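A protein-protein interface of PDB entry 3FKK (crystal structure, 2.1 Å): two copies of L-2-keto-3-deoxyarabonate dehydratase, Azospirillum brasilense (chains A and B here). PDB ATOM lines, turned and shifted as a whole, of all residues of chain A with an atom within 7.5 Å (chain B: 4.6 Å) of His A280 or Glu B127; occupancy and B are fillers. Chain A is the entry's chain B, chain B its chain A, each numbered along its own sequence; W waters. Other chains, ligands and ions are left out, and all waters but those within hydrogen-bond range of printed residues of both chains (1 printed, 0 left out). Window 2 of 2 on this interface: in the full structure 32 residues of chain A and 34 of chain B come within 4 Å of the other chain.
The backbone NH (N) of Thr B89 is in hydrogen-bond range of the backbone carbonyl oxygen (O) of His A280 (3.2 Å).
OG1 of Thr B89 sits close to N of Pro A281 (3.3 Å).
ND1 of His A280 sits close to NH2 of Arg B131 (3.3 Å).
The backbone carbonyl oxygen (O) of Ala A57 sits at hydrogen-bond distance from the guanidinium group (NH1) of Arg A279 (2.9 Å).
The side-chain amide nitrogen (NE2) of Gln B124 sits at hydrogen-bond distance from the side-chain carboxylate (OE1) of Glu B127.
Among the printed residues, merely in contact across the chains: His A280 with Glu B127, Pro A281 with Tyr B87, Pro A281 with Gln B124, Met A282 with Tyr B87, Ala A57 with Ser B88, His A280 with Ser B88, His A280 with Phe B128 and His A280 with Gln B124.
Gly A24 touches none of the printed residues of chain B.
Of the printed residues of chain B, Ala A57 touches Ser B88 (3.4 Å).
Of chain B, only Ser B88 (3.7 Å), Thr B89 (2.9 Å), Gln B124 (3.9 Å), Glu B127 (2.8 Å), Phe B128 (3.8 Å) and Arg B131 (3.3 Å) come within 4 Å of His A280.
Of the printed residues of chain B, Pro A281 touches Tyr B87, Thr B89 and Gln B124.
Printed residues of chain B within 4 Å of Met A282: Tyr B87 (3.3 Å).
Glu B127 touches one residue of chain A.
Of the printed residues of chain A, Arg B131 touches His A280.
Of the 13 printed residues of chain A, 4 touch a printed residue of chain B.
Hydrophobic or aromatic side chains of chain A that line the printed part of chain B: His A280, Pro A281 and Met A282.
Hydrophobic or aromatic side chains of chain B that line the printed part of chain A: Tyr B87.
Among the printed residues, no Asp or Glu carboxylate lies within 4 Å of a Lys or Arg side-chain nitrogen of the other chain.
No position is printed for both chains.
Of the 11 pairs that touch across the chains among the printed residues, none has its exchanged pair printed and touching as well.
Water W1 lies within hydrogen-bond range of the backbone carbonyl oxygen (O) of His A280, the side-chain hydroxyl (OG) of Ser B88 and the backbone NH (N) of Thr B89.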
ATOM      1  N   PHE A  20      16.609   2.421  -2.659  1.00  0.00           N
ATOM      2  CA  PHE A  20      15.583   3.353  -3.113  1.00  0.00           C
ATOM      3  C   PHE A  20      15.535   3.382  -4.630  1.00  0.00           C
ATOM      4  O   PHE A  20      16.496   3.003  -5.300  1.00  0.00           O
ATOM      5  CB  PHE A  20      15.877   4.786  -2.646  1.00  0.00           C
ATOM      6  CG  PHE A  20      16.013   4.937  -1.159  1.00  0.00           C
ATOM      7  CD1 PHE A  20      17.255   5.189  -0.586  1.00  0.00           C
ATOM      8  CD2 PHE A  20      14.898   4.845  -0.332  1.00  0.00           C
ATOM      9  CE1 PHE A  20      17.387   5.349   0.793  1.00  0.00           C
ATOM     10  CE2 PHE A  20      15.017   5.005   1.049  1.00  0.00           C
ATOM     11  CZ  PHE A  20      16.260   5.258   1.613  1.00  0.00           C
ATOM     12  N   THR A  23      13.895   8.019  -7.710  1.00  0.00           N
ATOM     13  CA  THR A  23      13.153   9.139  -7.145  1.00  0.00           C
ATOM     14  C   THR A  23      12.946   9.136  -5.626  1.00  0.00           C
ATOM     15  O   THR A  23      12.207   9.971  -5.105  1.00  0.00           O
ATOM     16  CB  THR A  23      11.789   9.285  -7.840  1.00  0.00           C
ATOM     17  OG1 THR A  23      11.154   8.004  -7.923  1.00  0.00           O
ATOM     18  CG2 THR A  23      11.975   9.842  -9.250  1.00  0.00           C
ATOM     19  N   GLY A  24      13.584   8.205  -4.920  1.00  0.00           N
ATOM     20  CA  GLY A  24      13.464   8.174  -3.468  1.00  0.00           C
ATOM     21  C   GLY A  24      12.512   7.169  -2.842  1.00  0.00           C
ATOM     22  O   GLY A  24      12.581   6.912  -1.638  1.00  0.00           O
ATOM     23  N   GLU A  54      20.599   3.894   6.252  1.00  0.00           N
ATOM     24  CA  GLU A  54      19.952   5.195   6.095  1.00  0.00           C
ATOM     25  C   GLU A  54      18.601   5.211   6.802  1.00  0.00           C
ATOM     26  O   GLU A  54      17.629   5.780   6.299  1.00  0.00           O
ATOM     27  CB  GLU A  54      19.753   5.520   4.613  1.00  0.00           C
ATOM     28  CG  GLU A  54      21.041   5.764   3.853  1.00  0.00           C
ATOM     29  CD  GLU A  54      20.816   5.857   2.359  1.00  0.00           C
ATOM     30  OE1 GLU A  54      20.183   6.836   1.902  1.00  0.00           O
ATOM     31  OE2 GLU A  54      21.264   4.939   1.643  1.00  0.00           O
ATOM     32  N   ALA A  57      16.487   8.331   7.280  1.00  0.00           N
ATOM     33  CA  ALA A  57      15.794   8.921   6.139  1.00  0.00           C
ATOM     34  C   ALA A  57      14.438   8.288   5.821  1.00  0.00           C
ATOM     35  O   ALA A  57      13.779   8.695   4.863  1.00  0.00           O
ATOM     36  CB  ALA A  57      16.696   8.865   4.897  1.00  0.00           C
ATOM     37  N   ARG A 277      21.389   5.526  -5.406  1.00  0.00           N
ATOM     38  CA  ARG A 277      21.129   6.821  -4.806  1.00  0.00           C
ATOM     39  C   ARG A 277      20.580   6.779  -3.389  1.00  0.00           C
ATOM     40  O   ARG A 277      19.847   5.863  -3.008  1.00  0.00           O
ATOM     41  CB  ARG A 277      20.170   7.622  -5.684  1.00  0.00           C
ATOM     42  CG  ARG A 277      20.687   7.854  -7.093  1.00  0.00           C
ATOM     43  CD  ARG A 277      19.737   8.720  -7.892  1.00  0.00           C
ATOM     44  NE  ARG A 277      19.570  10.037  -7.288  1.00  0.00           N
ATOM     45  CZ  ARG A 277      18.868  11.024  -7.839  1.00  0.00           C
ATOM     46  NH1 ARG A 277      18.267  10.839  -9.008  1.00  0.00           N
ATOM     47  NH2 ARG A 277      18.769  12.195  -7.223  1.00  0.00           N
ATOM     48  N   PRO A 278      20.964   7.769  -2.574  1.00  0.00           N
ATOM     49  CA  PRO A 278      20.495   7.859  -1.194  1.00  0.00           C
ATOM     50  C   PRO A 278      19.254   8.731  -1.290  1.00  0.00           C
ATOM     51  O   PRO A 278      18.881   9.150  -2.384  1.00  0.00           O
ATOM     52  CB  PRO A 278      21.631   8.591  -0.502  1.00  0.00           C
ATOM     53  CG  PRO A 278      22.018   9.605  -1.553  1.00  0.00           C
ATOM     54  CD  PRO A 278      22.018   8.769  -2.837  1.00  0.00           C
ATOM     55  N   ARG A 279      18.608   9.002  -0.167  1.00  0.00           N
ATOM     56  CA  ARG A 279      17.459   9.886  -0.203  1.00  0.00           C
ATOM     57  C   ARG A 279      17.985  11.296   0.009  1.00  0.00           C
ATOM     58  O   ARG A 279      18.886  11.507   0.824  1.00  0.00           O
ATOM     59  CB  ARG A 279      16.456   9.539   0.898  1.00  0.00           C
ATOM     60  CG  ARG A 279      15.222   8.856   0.366  1.00  0.00           C
ATOM     61  CD  ARG A 279      14.216   8.541   1.459  1.00  0.00           C
ATOM     62  NE  ARG A 279      13.111   7.770   0.905  1.00  0.00           N
ATOM     63  CZ  ARG A 279      12.097   7.282   1.610  1.00  0.00           C
ATOM     64  NH1 ARG A 279      12.027   7.486   2.921  1.00  0.00           N
ATOM     65  NH2 ARG A 279      11.164   6.567   0.999  1.00  0.00           N
ATOM     66  N   HIS A 280      17.451  12.251  -0.747  1.00  0.00           N
ATOM     67  CA  HIS A 280      17.856  13.645  -0.598  1.00  0.00           C
ATOM     68  C   HIS A 280      17.503  13.970   0.854  1.00  0.00           C
ATOM     69  O   HIS A 280      16.518  13.451   1.379  1.00  0.00           O
ATOM     70  CB  HIS A 280      17.048  14.530  -1.555  1.00  0.00           C
ATOM     71  CG  HIS A 280      17.567  15.932  -1.674  1.00  0.00           C
ATOM     72  ND1 HIS A 280      18.689  16.253  -2.411  1.00  0.00           N
ATOM     73  CD2 HIS A 280      17.121  17.095  -1.143  1.00  0.00           C
ATOM     74  CE1 HIS A 280      18.908  17.554  -2.331  1.00  0.00           C
ATOM     75  NE2 HIS A 280      17.972  18.088  -1.567  1.00  0.00           N
ATOM     76  N   PRO A 281      18.263  14.855   1.515  1.00  0.00           N
ATOM     77  CA  PRO A 281      19.435  15.628   1.093  1.00  0.00           C
ATOM     78  C   PRO A 281      20.809  14.953   1.157  1.00  0.00           C
ATOM     79  O   PRO A 281      21.817  15.612   0.908  1.00  0.00           O
ATOM     80  CB  PRO A 281      19.375  16.835   2.015  1.00  0.00           C
ATOM     81  CG  PRO A 281      19.001  16.189   3.311  1.00  0.00           C
ATOM     82  CD  PRO A 281      17.901  15.201   2.902  1.00  0.00           C
ATOM     83  N   MET A 282      20.880  13.668   1.484  1.00  0.00           N
ATOM     84  CA  MET A 282      22.198  13.037   1.538  1.00  0.00           C
ATOM     85  C   MET A 282      22.871  13.208   0.180  1.00  0.00           C
ATOM     86  O   MET A 282      22.282  12.915  -0.861  1.00  0.00           O
ATOM     87  CB  MET A 282      22.099  11.556   1.894  1.00  0.00           C
ATOM     88  CG  MET A 282      23.445  10.957   2.259  1.00  0.00           C
ATOM     89  SD  MET A 282      23.330   9.338   3.040  1.00  0.00           S
ATOM     90  CE  MET A 282      24.166   8.362   1.850  1.00  0.00           C
ATOM     91  N   PRO A 283      24.118  13.700   0.172  1.00  0.00           N
ATOM     92  CA  PRO A 283      24.830  13.903  -1.089  1.00  0.00           C
ATOM     93  C   PRO A 283      25.249  12.622  -1.802  1.00  0.00           C
ATOM     94  O   PRO A 283      25.537  11.601  -1.172  1.00  0.00           O
ATOM     95  CB  PRO A 283      26.024  14.753  -0.668  1.00  0.00           C
ATOM     96  CG  PRO A 283      26.339  14.215   0.688  1.00  0.00           C
ATOM     97  CD  PRO A 283      24.968  14.059   1.323  1.00  0.00           C
ATOM     98  N   GLU A 284      25.266  12.693  -3.127  1.00  0.00           N
ATOM     99  CA  GLU A 284      25.676  11.572  -3.963  1.00  0.00           C
ATOM    100  C   GLU A 284      27.188  11.468  -3.790  1.00  0.00           C
ATOM    101  O   GLU A 284      27.822  12.398  -3.291  1.00  0.00           O
ATOM    102  CB  GLU A 284      25.369  11.870  -5.434  1.00  0.00           C
ATOM    103  CG  GLU A 284      23.902  12.140  -5.742  1.00  0.00           C
ATOM    104  CD  GLU A 284      23.065  10.874  -5.754  1.00  0.00           C
ATOM    105  OE1 GLU A 284      21.832  10.979  -5.933  1.00  0.00           O
ATOM    106  OE2 GLU A 284      23.640   9.776  -5.592  1.00  0.00           O
ATOM    107  N   TYR B  87      15.196  14.392   8.539  1.00  0.00           N
ATOM    108  CA  TYR B  87      16.362  14.364   7.668  1.00  0.00           C
ATOM    109  C   TYR B  87      15.940  14.316   6.204  1.00  0.00           C
ATOM    110  O   TYR B  87      16.469  15.052   5.378  1.00  0.00           O
ATOM    111  CB  TYR B  87      17.243  13.161   8.007  1.00  0.00           C
ATOM    112  CG  TYR B  87      18.509  13.069   7.185  1.00  0.00           C
ATOM    113  CD1 TYR B  87      18.482  12.588   5.874  1.00  0.00           C
ATOM    114  CD2 TYR B  87      19.738  13.464   7.719  1.00  0.00           C
ATOM    115  CE1 TYR B  87      19.650  12.497   5.117  1.00  0.00           C
ATOM    116  CE2 TYR B  87      20.910  13.381   6.969  1.00  0.00           C
ATOM    117  CZ  TYR B  87      20.858  12.894   5.671  1.00  0.00           C
ATOM    118  OH  TYR B  87      22.017  12.788   4.935  1.00  0.00           O
ATOM    119  N   SER B  88      14.975  13.460   5.886  1.00  0.00           N
ATOM    120  CA  SER B  88      14.499  13.323   4.517  1.00  0.00           C
ATOM    121  C   SER B  88      13.725  14.541   4.009  1.00  0.00           C
ATOM    122  O   SER B  88      12.722  14.947   4.595  1.00  0.00           O
ATOM    123  CB  SER B  88      13.623  12.075   4.393  1.00  0.00           C
ATOM    124  OG  SER B  88      12.889  12.078   3.181  1.00  0.00           O
ATOM    125  N   THR B  89      14.195  15.107   2.903  1.00  0.00           N
ATOM    126  CA  THR B  89      13.554  16.266   2.297  1.00  0.00           C
ATOM    127  C   THR B  89      12.106  15.964   1.932  1.00  0.00           C
ATOM    128  O   THR B  89      11.197  16.735   2.238  1.00  0.00           O
ATOM    129  CB  THR B  89      14.296  16.692   1.020  1.00  0.00           C
ATOM    130  OG1 THR B  89      15.673  16.924   1.333  1.00  0.00           O
ATOM    131  CG2 THR B  89      13.694  17.966   0.447  1.00  0.00           C
ATOM    132  N   ALA B 123      25.181  23.130   0.314  1.00  0.00           N
ATOM    133  CA  ALA B 123      24.502  22.980  -0.968  1.00  0.00           C
ATOM    134  C   ALA B 123      23.247  22.109  -0.866  1.00  0.00           C
ATOM    135  O   ALA B 123      22.216  22.437  -1.449  1.00  0.00           O
ATOM    136  CB  ALA B 123      25.465  22.394  -2.005  1.00  0.00           C
ATOM    137  N   GLN B 124      23.335  21.000  -0.135  1.00  0.00           N
ATOM    138  CA  GLN B 124      22.186  20.109   0.008  1.00  0.00           C
ATOM    139  C   GLN B 124      21.178  20.673   1.011  1.00  0.00           C
ATOM    140  O   GLN B 124      19.977  20.453   0.875  1.00  0.00           O
ATOM    141  CB  GLN B 124      22.635  18.715   0.455  1.00  0.00           C
ATOM    142  CG  GLN B 124      24.057  18.356   0.055  1.00  0.00           C
ATOM    143  CD  GLN B 124      24.312  18.458  -1.435  1.00  0.00           C
ATOM    144  OE1 GLN B 124      25.461  18.533  -1.867  1.00  0.00           O
ATOM    145  NE2 GLN B 124      23.245  18.449  -2.230  1.00  0.00           N
ATOM    146  N   ILE B 125      21.662  21.393   2.020  1.00  0.00           N
ATOM    147  CA  ILE B 125      20.765  22.000   3.002  1.00  0.00           C
ATOM    148  C   ILE B 125      19.899  23.019   2.263  1.00  0.00           C
ATOM    149  O   ILE B 125      18.686  23.096   2.472  1.00  0.00           O
ATOM    150  CB  ILE B 125      21.554  22.714   4.138  1.00  0.00           C
ATOM    151  CG1 ILE B 125      22.218  21.673   5.042  1.00  0.00           C
ATOM    152  CG2 ILE B 125      20.617  23.608   4.952  1.00  0.00           C
ATOM    153  CD1 ILE B 125      23.015  22.267   6.191  1.00  0.00           C
ATOM    154  N   PHE B 126      20.533  23.792   1.385  1.00  0.00           N
ATOM    155  CA  PHE B 126      19.827  24.795   0.597  1.00  0.00           C
ATOM    156  C   PHE B 126      18.746  24.120  -0.246  1.00  0.00           C
ATOM    157  O   PHE B 126      17.618  24.611  -0.330  1.00  0.00           O
ATOM    158  CB  PHE B 126      20.818  25.546  -0.304  1.00  0.00           C
ATOM    159  CG  PHE B 126      20.191  26.656  -1.102  1.00  0.00           C
ATOM    160  CD1 PHE B 126      19.412  26.377  -2.223  1.00  0.00           C
ATOM    161  CD2 PHE B 126      20.362  27.985  -0.719  1.00  0.00           C
ATOM    162  CE1 PHE B 126      18.811  27.403  -2.952  1.00  0.00           C
ATOM    163  CE2 PHE B 126      19.766  29.021  -1.440  1.00  0.00           C
ATOM    164  CZ  PHE B 126      18.988  28.728  -2.560  1.00  0.00           C
ATOM    165  N   GLU B 127      19.092  22.990  -0.864  1.00  0.00           N
ATOM    166  CA  GLU B 127      18.141  22.242  -1.686  1.00  0.00           C
ATOM    167  C   GLU B 127      17.014  21.680  -0.811  1.00  0.00           C
ATOM    168  O   GLU B 127      15.861  21.608  -1.230  1.00  0.00           O
ATOM    169  CB  GLU B 127      18.856  21.096  -2.418  1.00  0.00           C
ATOM    170  CG  GLU B 127      20.085  21.548  -3.207  1.00  0.00           C
ATOM    171  CD  GLU B 127      20.734  20.430  -4.007  1.00  0.00           C
ATOM    172  OE1 GLU B 127      20.798  19.285  -3.508  1.00  0.00           O
ATOM    173  OE2 GLU B 127      21.198  20.706  -5.135  1.00  0.00           O
ATOM    174  N   PHE B 128      17.361  21.269   0.403  1.00  0.00           N
ATOM    175  CA  PHE B 128      16.374  20.737   1.337  1.00  0.00           C
ATOM    176  C   PHE B 128      15.280  21.785   1.528  1.00  0.00           C
ATOM    177  O   PHE B 128      14.108  21.524   1.266  1.00  0.00           O
ATOM    178  CB  PHE B 128      17.051  20.401   2.679  1.00  0.00           C
ATOM    179  CG  PHE B 128      16.090  20.043   3.793  1.00  0.00           C
ATOM    180  CD1 PHE B 128      15.535  21.033   4.602  1.00  0.00           C
ATOM    181  CD2 PHE B 128      15.757  18.714   4.043  1.00  0.00           C
ATOM    182  CE1 PHE B 128      14.665  20.706   5.648  1.00  0.00           C
ATOM    183  CE2 PHE B 128      14.886  18.373   5.087  1.00  0.00           C
ATOM    184  CZ  PHE B 128      14.339  19.371   5.890  1.00  0.00           C
ATOM    185  N   TYR B 129      15.670  22.983   1.961  1.00  0.00           N
ATOM    186  CA  TYR B 129      14.703  24.052   2.182  1.00  0.00           C
ATOM    187  C   TYR B 129      14.008  24.525   0.911  1.00  0.00           C
ATOM    188  O   TYR B 129      12.819  24.840   0.933  1.00  0.00           O
ATOM    189  CB  TYR B 129      15.375  25.237   2.877  1.00  0.00           C
ATOM    190  CG  TYR B 129      15.642  24.999   4.349  1.00  0.00           C
ATOM    191  CD1 TYR B 129      14.588  24.842   5.253  1.00  0.00           C
ATOM    192  CD2 TYR B 129      16.945  24.914   4.836  1.00  0.00           C
ATOM    193  CE1 TYR B 129      14.826  24.604   6.603  1.00  0.00           C
ATOM    194  CE2 TYR B 129      17.197  24.677   6.183  1.00  0.00           C
ATOM    195  CZ  TYR B 129      16.134  24.525   7.062  1.00  0.00           C
ATOM    196  OH  TYR B 129      16.390  24.315   8.396  1.00  0.00           O
ATOM    197  N   ALA B 130      14.739  24.575  -0.195  1.00  0.00           N
ATOM    198  CA  ALA B 130      14.157  25.013  -1.460  1.00  0.00           C
ATOM    199  C   ALA B 130      13.023  24.085  -1.883  1.00  0.00           C
ATOM    200  O   ALA B 130      11.969  24.531  -2.336  1.00  0.00           O
ATOM    201  CB  ALA B 130      15.234  25.054  -2.546  1.00  0.00           C
ATOM    202  N   ARG B 131      13.240  22.787  -1.723  1.00  0.00           N
ATOM    203  CA  ARG B 131      12.236  21.812  -2.102  1.00  0.00           C
ATOM    204  C   ARG B 131      11.059  21.792  -1.136  1.00  0.00           C
ATOM    205  O   ARG B 131       9.921  21.585  -1.553  1.00  0.00           O
ATOM    206  CB  ARG B 131      12.885  20.436  -2.236  1.00  0.00           C
ATOM    207  CG  ARG B 131      13.983  20.459  -3.286  1.00  0.00           C
ATOM    208  CD  ARG B 131      14.619  19.115  -3.526  1.00  0.00           C
ATOM    209  NE  ARG B 131      15.741  19.247  -4.452  1.00  0.00           N
ATOM    210  CZ  ARG B 131      16.491  18.234  -4.872  1.00  0.00           C
ATOM    211  NH1 ARG B 131      17.492  18.457  -5.712  1.00  0.00           N
ATOM    212  NH2 ARG B 131      16.237  17.001  -4.453  1.00  0.00           N
HETATM  213  O   HOH W   1      14.070  12.651   0.598  1.00  0.00           O
